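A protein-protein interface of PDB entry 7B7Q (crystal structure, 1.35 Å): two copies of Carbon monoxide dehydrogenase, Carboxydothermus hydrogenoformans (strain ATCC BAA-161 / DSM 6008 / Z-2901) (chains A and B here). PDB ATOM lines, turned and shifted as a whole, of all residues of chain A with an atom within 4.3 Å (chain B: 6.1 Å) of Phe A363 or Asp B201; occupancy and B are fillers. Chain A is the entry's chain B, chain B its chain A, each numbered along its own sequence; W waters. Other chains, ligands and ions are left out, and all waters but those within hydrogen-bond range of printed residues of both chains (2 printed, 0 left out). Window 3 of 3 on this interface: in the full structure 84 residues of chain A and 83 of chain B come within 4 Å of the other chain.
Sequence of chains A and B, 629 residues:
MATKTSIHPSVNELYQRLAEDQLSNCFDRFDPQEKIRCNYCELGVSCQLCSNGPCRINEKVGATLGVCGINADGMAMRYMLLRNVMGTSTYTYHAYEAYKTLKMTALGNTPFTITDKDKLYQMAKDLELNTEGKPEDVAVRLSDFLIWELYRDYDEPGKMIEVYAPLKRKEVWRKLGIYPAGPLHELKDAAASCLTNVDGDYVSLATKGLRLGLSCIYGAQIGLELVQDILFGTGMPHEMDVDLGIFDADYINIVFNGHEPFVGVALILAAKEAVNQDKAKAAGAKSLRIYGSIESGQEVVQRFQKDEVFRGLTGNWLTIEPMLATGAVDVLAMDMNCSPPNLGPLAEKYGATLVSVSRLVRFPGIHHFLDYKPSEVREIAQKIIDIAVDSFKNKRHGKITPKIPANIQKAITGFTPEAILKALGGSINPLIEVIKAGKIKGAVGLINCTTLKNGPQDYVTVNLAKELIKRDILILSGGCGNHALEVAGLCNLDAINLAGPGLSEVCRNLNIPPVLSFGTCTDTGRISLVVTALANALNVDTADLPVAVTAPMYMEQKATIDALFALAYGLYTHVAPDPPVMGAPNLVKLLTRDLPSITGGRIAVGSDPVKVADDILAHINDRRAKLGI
Among the printed residues, merely in contact across the chains: Pro A341 with Ile B70, Arg A362 with Val B198, Arg A362 with Asp B201, Arg A362 with Ser B204, Phe A363 with Asp B201 and Pro A364 with Gly B200.
Along chain A the printed residues that touch a printed residue of chain B span positions 341 to 364.
Of the 12 printed residues of chain B, 6 touch a printed residue of chain A.
Hydrophobic or aromatic side chains of chain B that line the printed part of chain A: Ile B70.
Among the printed residues, no Asp or Glu carboxylate lies within 4 Å of a Lys or Arg side-chain nitrogen of the other chain.
Water W1 lies within hydrogen-bond range of O of Ser A339 (2.8 Å) and O of Val B198 (2.9 Å).
Water W2 lies within hydrogen-bond range of OD2 of Asp B201 and O of Phe A363.
O of Arg A362 is in hydrogen-bond range of N of Gly B200 (2.9 Å).
The backbone carbonyl oxygen (O) of Arg A362 lies close to the side-chain carboxylate (OD1) of Asp B199 (3.4 Å).
Of the printed residues of chain B, Phe A363 touches Asp B201.
Of the printed residues of chain A, Asp B201 touches Arg A362 and Phe A363.
Printed residues of chain B within 4 Å of Pro A364: Gly B200.
Printed residues of chain A within 4 Å of Gly B200: Arg A362 (2.9 Å) and Pro A364 (3.98 Å).
Of the printed residues of chain A, Ile B70 touches Pro A341 (3.5 Å).
Of the printed residues of chain B, Pro A341 touches Ile B70 (3.5 Å).
Printed residues of chain B within 4 Å of Arg A362: Val B198 (3.5 Å), Asp B199 (3.4 Å), Gly B200 (2.9 Å), Asp B201 (3.7 Å) and Ser B204 (3.5 Å).
Gly A365 touches none of the printed residues of chain B.
Leu A343 touches none of the printed residues of chain B.
The nearest printed residue of chain A that does not touch Asp B201 is Pro A364 (4.1 Å).
OD1 of Asp B199 is in hydrogen-bond range of N of Asp B201 (3.0 Å).
The side-chain hydroxyl of Ser B204 is in hydrogen-bond range of the side-chain carboxylate of Asp B199, 2.7 Å away.
OD1 of Asp B201 sits at hydrogen-bond distance from N of Val B203 (3.1 Å).
OD1 of Asp B201 lies within hydrogen-bond range of N of Ser B204 (3.1 Å).
No position is printed for both chains.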
ATOM      1  N   MET A 334     -11.062 -19.051  23.045  1.00  0.00           N
ATOM      2  CA  MET A 334     -11.804 -17.809  22.798  1.00  0.00           C
ATOM      3  C   MET A 334     -12.970 -18.059  21.852  1.00  0.00           C
ATOM      4  O   MET A 334     -12.767 -18.550  20.737  1.00  0.00           O
ATOM      5  CB  MET A 334     -10.875 -16.779  22.157  1.00  0.00           C
ATOM      6  CG  MET A 334      -9.650 -16.461  22.985  1.00  0.00           C
ATOM      7  SD  MET A 334      -8.311 -15.609  22.117  1.00  0.00           S
ATOM      8  CE  MET A 334      -7.807 -16.886  20.961  1.00  0.00           C
ATOM      9  N   SER A 339     -12.030 -10.751  22.432  1.00  0.00           N
ATOM     10  CA  SER A 339     -10.748 -11.420  22.218  1.00  0.00           C
ATOM     11  C   SER A 339      -9.814 -10.409  21.549  1.00  0.00           C
ATOM     12  O   SER A 339      -9.767 -10.308  20.307  1.00  0.00           O
ATOM     13  CB  SER A 339     -10.950 -12.662  21.363  1.00  0.00           C
ATOM     14  OG  SER A 339     -11.819 -13.589  22.043  1.00  0.00           O
ATOM     15  N   PRO A 340      -9.094  -9.589  22.321  1.00  0.00           N
ATOM     16  CA  PRO A 340      -8.393  -8.443  21.737  1.00  0.00           C
ATOM     17  C   PRO A 340      -7.296  -8.890  20.786  1.00  0.00           C
ATOM     18  O   PRO A 340      -6.596  -9.884  21.047  1.00  0.00           O
ATOM     19  CB  PRO A 340      -7.816  -7.724  22.967  1.00  0.00           C
ATOM     20  CG  PRO A 340      -8.735  -8.106  24.097  1.00  0.00           C
ATOM     21  CD  PRO A 340      -9.062  -9.546  23.793  1.00  0.00           C
ATOM     22  N   PRO A 341      -7.124  -8.208  19.646  1.00  0.00           N
ATOM     23  CA  PRO A 341      -6.348  -8.811  18.551  1.00  0.00           C
ATOM     24  C   PRO A 341      -4.830  -8.717  18.660  1.00  0.00           C
ATOM     25  O   PRO A 341      -4.151  -9.186  17.740  1.00  0.00           O
ATOM     26  CB  PRO A 341      -6.842  -8.046  17.320  1.00  0.00           C
ATOM     27  CG  PRO A 341      -7.313  -6.714  17.873  1.00  0.00           C
ATOM     28  CD  PRO A 341      -7.921  -7.050  19.185  1.00  0.00           C
ATOM     29  N   LEU A 343      -3.158 -10.141  21.363  1.00  0.00           N
ATOM     30  CA  LEU A 343      -2.741 -11.061  22.419  1.00  0.00           C
ATOM     31  C   LEU A 343      -1.543 -11.918  22.035  1.00  0.00           C
ATOM     32  O   LEU A 343      -0.895 -12.477  22.929  1.00  0.00           O
ATOM     33  CB  LEU A 343      -3.876 -11.996  22.863  1.00  0.00           C
ATOM     34  CG  LEU A 343      -5.108 -11.369  23.513  1.00  0.00           C
ATOM     35  CD1 LEU A 343      -6.075 -12.458  23.905  1.00  0.00           C
ATOM     36  CD2 LEU A 343      -4.736 -10.465  24.704  1.00  0.00           C
ATOM     37  N   GLY A 344      -1.270 -12.074  20.744  1.00  0.00           N
ATOM     38  CA  GLY A 344      -0.228 -12.962  20.284  1.00  0.00           C
ATOM     39  C   GLY A 344       1.113 -12.773  20.971  1.00  0.00           C
ATOM     40  O   GLY A 344       1.668 -13.720  21.528  1.00  0.00           O
ATOM     41  N   LEU A 354      -2.957 -19.986  22.515  1.00  0.00           N
ATOM     42  CA  LEU A 354      -4.223 -19.375  22.138  1.00  0.00           C
ATOM     43  C   LEU A 354      -4.989 -20.290  21.181  1.00  0.00           C
ATOM     44  O   LEU A 354      -4.433 -20.758  20.169  1.00  0.00           O
ATOM     45  CB  LEU A 354      -3.935 -18.033  21.458  1.00  0.00           C
ATOM     46  CG  LEU A 354      -3.167 -16.968  22.240  1.00  0.00           C
ATOM     47  CD1 LEU A 354      -2.922 -15.744  21.353  1.00  0.00           C
ATOM     48  CD2 LEU A 354      -3.922 -16.572  23.502  1.00  0.00           C
ATOM     49  N   ARG A 362     -10.680 -14.428  14.901  1.00  0.00           N
ATOM     50  CA  ARG A 362      -9.380 -14.589  14.256  1.00  0.00           C
ATOM     51  C   ARG A 362      -8.582 -13.317  14.538  1.00  0.00           C
ATOM     52  O   ARG A 362      -9.151 -12.232  14.595  1.00  0.00           O
ATOM     53  CB  ARG A 362      -9.531 -14.757  12.731  1.00  0.00           C
ATOM     54  CG  ARG A 362     -10.274 -15.989  12.282  1.00  0.00           C
ATOM     55  CD  ARG A 362      -9.511 -17.260  12.589  1.00  0.00           C
ATOM     56  NE  ARG A 362     -10.041 -18.485  11.999  1.00  0.00           N
ATOM     57  CZ  ARG A 362     -10.949 -19.286  12.553  1.00  0.00           C
ATOM     58  NH1 ARG A 362     -11.479 -18.978  13.726  1.00  0.00           N
ATOM     59  NH2 ARG A 362     -11.321 -20.404  11.934  1.00  0.00           N
ATOM     60  N   PHE A 363      -7.258 -13.460  14.694  1.00  0.00           N
ATOM     61  CA  PHE A 363      -6.301 -12.361  14.843  1.00  0.00           C
ATOM     62  C   PHE A 363      -4.898 -12.954  14.769  1.00  0.00           C
ATOM     63  O   PHE A 363      -4.742 -14.168  14.847  1.00  0.00           O
ATOM     64  CB  PHE A 363      -6.534 -11.536  16.143  1.00  0.00           C
ATOM     65  CG  PHE A 363      -6.416 -12.299  17.452  1.00  0.00           C
ATOM     66  CD1 PHE A 363      -5.162 -12.578  17.993  1.00  0.00           C
ATOM     67  CD2 PHE A 363      -7.542 -12.641  18.170  1.00  0.00           C
ATOM     68  CE1 PHE A 363      -5.051 -13.233  19.205  1.00  0.00           C
ATOM     69  CE2 PHE A 363      -7.443 -13.288  19.390  1.00  0.00           C
ATOM     70  CZ  PHE A 363      -6.204 -13.597  19.905  1.00  0.00           C
ATOM     71  N   PRO A 364      -3.860 -12.125  14.567  1.00  0.00           N
ATOM     72  CA  PRO A 364      -2.508 -12.681  14.362  1.00  0.00           C
ATOM     73  C   PRO A 364      -2.007 -13.490  15.561  1.00  0.00           C
ATOM     74  O   PRO A 364      -2.186 -13.105  16.717  1.00  0.00           O
ATOM     75  CB  PRO A 364      -1.645 -11.440  14.121  1.00  0.00           C
ATOM     76  CG  PRO A 364      -2.607 -10.380  13.624  1.00  0.00           C
ATOM     77  CD  PRO A 364      -3.899 -10.665  14.338  1.00  0.00           C
ATOM     78  N   GLY A 365      -1.371 -14.612  15.283  1.00  0.00           N
ATOM     79  CA  GLY A 365      -0.662 -15.359  16.314  1.00  0.00           C
ATOM     80  C   GLY A 365      -1.472 -16.397  17.070  1.00  0.00           C
ATOM     81  O   GLY A 365      -1.000 -16.900  18.100  1.00  0.00           O
ATOM     82  N   ILE A 366      -2.677 -16.736  16.605  1.00  0.00           N
ATOM     83  CA  ILE A 366      -3.445 -17.819  17.211  1.00  0.00           C
ATOM     84  C   ILE A 366      -2.812 -19.149  16.824  1.00  0.00           C
ATOM     85  O   ILE A 366      -2.361 -19.332  15.684  1.00  0.00           O
ATOM     86  CB  ILE A 366      -4.918 -17.715  16.773  1.00  0.00           C
ATOM     87  CG1 ILE A 366      -5.553 -16.463  17.396  1.00  0.00           C
ATOM     88  CG2 ILE A 366      -5.693 -18.985  17.166  1.00  0.00           C
ATOM     89  CD1 ILE A 366      -6.992 -16.173  16.940  1.00  0.00           C
ATOM     90  N   ILE B  70      -5.768  -3.612  17.291  1.00  0.00           N
ATOM     91  CA  ILE B  70      -5.860  -3.917  15.856  1.00  0.00           C
ATOM     92  C   ILE B  70      -4.840  -3.091  15.071  1.00  0.00           C
ATOM     93  O   ILE B  70      -4.573  -1.925  15.392  1.00  0.00           O
ATOM     94  CB  ILE B  70      -7.298  -3.735  15.327  1.00  0.00           C
ATOM     95  CG1 ILE B  70      -7.530  -4.513  14.005  1.00  0.00           C
ATOM     96  CG2 ILE B  70      -7.677  -2.250  15.166  1.00  0.00           C
ATOM     97  CD1 ILE B  70      -8.981  -4.597  13.571  1.00  0.00           C
ATOM     98  N   GLY B  74      -5.971  -4.815   9.458  1.00  0.00           N
ATOM     99  CA  GLY B  74      -7.247  -5.247  10.004  1.00  0.00           C
ATOM    100  C   GLY B  74      -8.267  -4.128  10.060  1.00  0.00           C
ATOM    101  O   GLY B  74      -9.448  -4.329   9.748  1.00  0.00           O
ATOM    102  N   MET B  77      -9.568  -3.428   6.359  1.00  0.00           N
ATOM    103  CA  MET B  77     -10.399  -4.498   5.801  1.00  0.00           C
ATOM    104  C   MET B  77     -11.695  -4.694   6.588  1.00  0.00           C
ATOM    105  O   MET B  77     -12.729  -5.054   6.001  1.00  0.00           O
ATOM    106  CB  MET B  77      -9.616  -5.802   5.711  1.00  0.00           C
ATOM    107  CG  MET B  77     -10.353  -6.902   4.910  1.00  0.00           C
ATOM    108  SD  MET B  77     -10.685  -6.493   3.175  1.00  0.00           S
ATOM    109  CE  MET B  77     -12.478  -6.778   3.073  1.00  0.00           C
ATOM    110  N   VAL B 198     -13.449  -9.108  17.913  1.00  0.00           N
ATOM    111  CA  VAL B 198     -13.931 -10.356  17.334  1.00  0.00           C
ATOM    112  C   VAL B 198     -12.914 -10.802  16.271  1.00  0.00           C
ATOM    113  O   VAL B 198     -11.986 -11.559  16.587  1.00  0.00           O
ATOM    114  CB  VAL B 198     -15.399 -10.270  16.824  1.00  0.00           C
ATOM    115  CG1 VAL B 198     -15.863 -11.621  16.279  1.00  0.00           C
ATOM    116  CG2 VAL B 198     -16.341  -9.821  17.953  1.00  0.00           C
ATOM    117  N   ASP B 199     -13.073 -10.360  15.001  1.00  0.00           N
ATOM    118  CA  ASP B 199     -12.107 -10.663  13.923  1.00  0.00           C
ATOM    119  C   ASP B 199     -11.242  -9.431  13.617  1.00  0.00           C
ATOM    120  O   ASP B 199     -11.748  -8.412  13.124  1.00  0.00           O
ATOM    121  CB  ASP B 199     -12.834 -11.153  12.668  1.00  0.00           C
ATOM    122  CG  ASP B 199     -11.908 -11.799  11.636  1.00  0.00           C
ATOM    123  OD1 ASP B 199     -10.695 -11.479  11.619  1.00  0.00           O
ATOM    124  OD2 ASP B 199     -12.424 -12.616  10.816  1.00  0.00           O
ATOM    125  N   GLY B 200      -9.950  -9.505  13.971  1.00  0.00           N
ATOM    126  CA  GLY B 200      -8.955  -8.480  13.709  1.00  0.00           C
ATOM    127  C   GLY B 200      -7.848  -8.934  12.765  1.00  0.00           C
ATOM    128  O   GLY B 200      -6.757  -8.366  12.782  1.00  0.00           O
ATOM    129  N   ASP B 201      -8.111  -9.948  11.936  1.00  0.00           N
ATOM    130  CA  ASP B 201      -7.125 -10.546  11.036  1.00  0.00           C
ATOM    131  C   ASP B 201      -7.469 -10.165   9.587  1.00  0.00           C
ATOM    132  O   ASP B 201      -8.468 -10.630   9.041  1.00  0.00           O
ATOM    133  CB  ASP B 201      -7.214 -12.058  11.231  1.00  0.00           C
ATOM    134  CG  ASP B 201      -6.186 -12.824  10.467  1.00  0.00           C
ATOM    135  OD1 ASP B 201      -6.130 -12.713   9.225  1.00  0.00           O
ATOM    136  OD2 ASP B 201      -5.438 -13.578  11.124  1.00  0.00           O
ATOM    137  N   TYR B 202      -6.645  -9.324   8.953  1.00  0.00           N
ATOM    138  CA  TYR B 202      -7.006  -8.809   7.631  1.00  0.00           C
ATOM    139  C   TYR B 202      -7.188  -9.914   6.589  1.00  0.00           C
ATOM    140  O   TYR B 202      -8.015  -9.763   5.679  1.00  0.00           O
ATOM    141  CB  TYR B 202      -6.011  -7.757   7.134  1.00  0.00           C
ATOM    142  CG  TYR B 202      -4.691  -8.307   6.606  1.00  0.00           C
ATOM    143  CD1 TYR B 202      -3.653  -8.631   7.472  1.00  0.00           C
ATOM    144  CD2 TYR B 202      -4.486  -8.497   5.246  1.00  0.00           C
ATOM    145  CE1 TYR B 202      -2.438  -9.144   6.993  1.00  0.00           C
ATOM    146  CE2 TYR B 202      -3.272  -8.991   4.747  1.00  0.00           C
ATOM    147  CZ  TYR B 202      -2.246  -9.328   5.634  1.00  0.00           C
ATOM    148  OH  TYR B 202      -1.033  -9.846   5.180  1.00  0.00           O
ATOM    149  N   VAL B 203      -6.437 -11.024   6.682  1.00  0.00           N
ATOM    150  CA  VAL B 203      -6.601 -12.111   5.707  1.00  0.00           C
ATOM    151  C   VAL B 203      -7.959 -12.793   5.895  1.00  0.00           C
ATOM    152  O   VAL B 203      -8.679 -13.074   4.928  1.00  0.00           O
ATOM    153  CB  VAL B 203      -5.441 -13.131   5.785  1.00  0.00           C
ATOM    154  CG1 VAL B 203      -5.634 -14.263   4.767  1.00  0.00           C
ATOM    155  CG2 VAL B 203      -4.097 -12.438   5.509  1.00  0.00           C
ATOM    156  N   SER B 204      -8.347 -13.039   7.153  1.00  0.00           N
ATOM    157  CA  SER B 204      -9.655 -13.614   7.465  1.00  0.00           C
ATOM    158  C   SER B 204     -10.790 -12.702   7.008  1.00  0.00           C
ATOM    159  O   SER B 204     -11.785 -13.162   6.429  1.00  0.00           O
ATOM    160  CB  SER B 204      -9.742 -13.842   8.969  1.00  0.00           C
ATOM    161  OG  SER B 204     -11.028 -14.298   9.286  1.00  0.00           O
ATOM    162  N   LEU B 205     -10.680 -11.404   7.311  1.00  0.00           N
ATOM    163  CA  LEU B 205     -11.703 -10.435   6.917  1.00  0.00           C
ATOM    164  C   LEU B 205     -11.846 -10.369   5.400  1.00  0.00           C
ATOM    165  O   LEU B 205     -12.969 -10.289   4.877  1.00  0.00           O
ATOM    166  CB  LEU B 205     -11.411  -9.067   7.536  1.00  0.00           C
ATOM    167  CG  LEU B 205     -11.465  -8.980   9.072  1.00  0.00           C
ATOM    168  CD1 LEU B 205     -10.609  -7.835   9.627  1.00  0.00           C
ATOM    169  CD2 LEU B 205     -12.932  -8.863   9.560  1.00  0.00           C
ATOM    170  N   ALA B 206     -10.727 -10.427   4.668  1.00  0.00           N
ATOM    171  CA  ALA B 206     -10.812 -10.430   3.214  1.00  0.00           C
ATOM    172  C   ALA B 206     -11.493 -11.699   2.721  1.00  0.00           C
ATOM    173  O   ALA B 206     -12.306 -11.659   1.796  1.00  0.00           O
ATOM    174  CB  ALA B 206      -9.413 -10.298   2.611  1.00  0.00           C
HETATM  175  O   HOH W   1      -9.848  -9.886  17.562  1.00  0.00           O
HETATM  176  O   HOH W   2      -6.147 -15.961  12.642  1.00  0.00           O
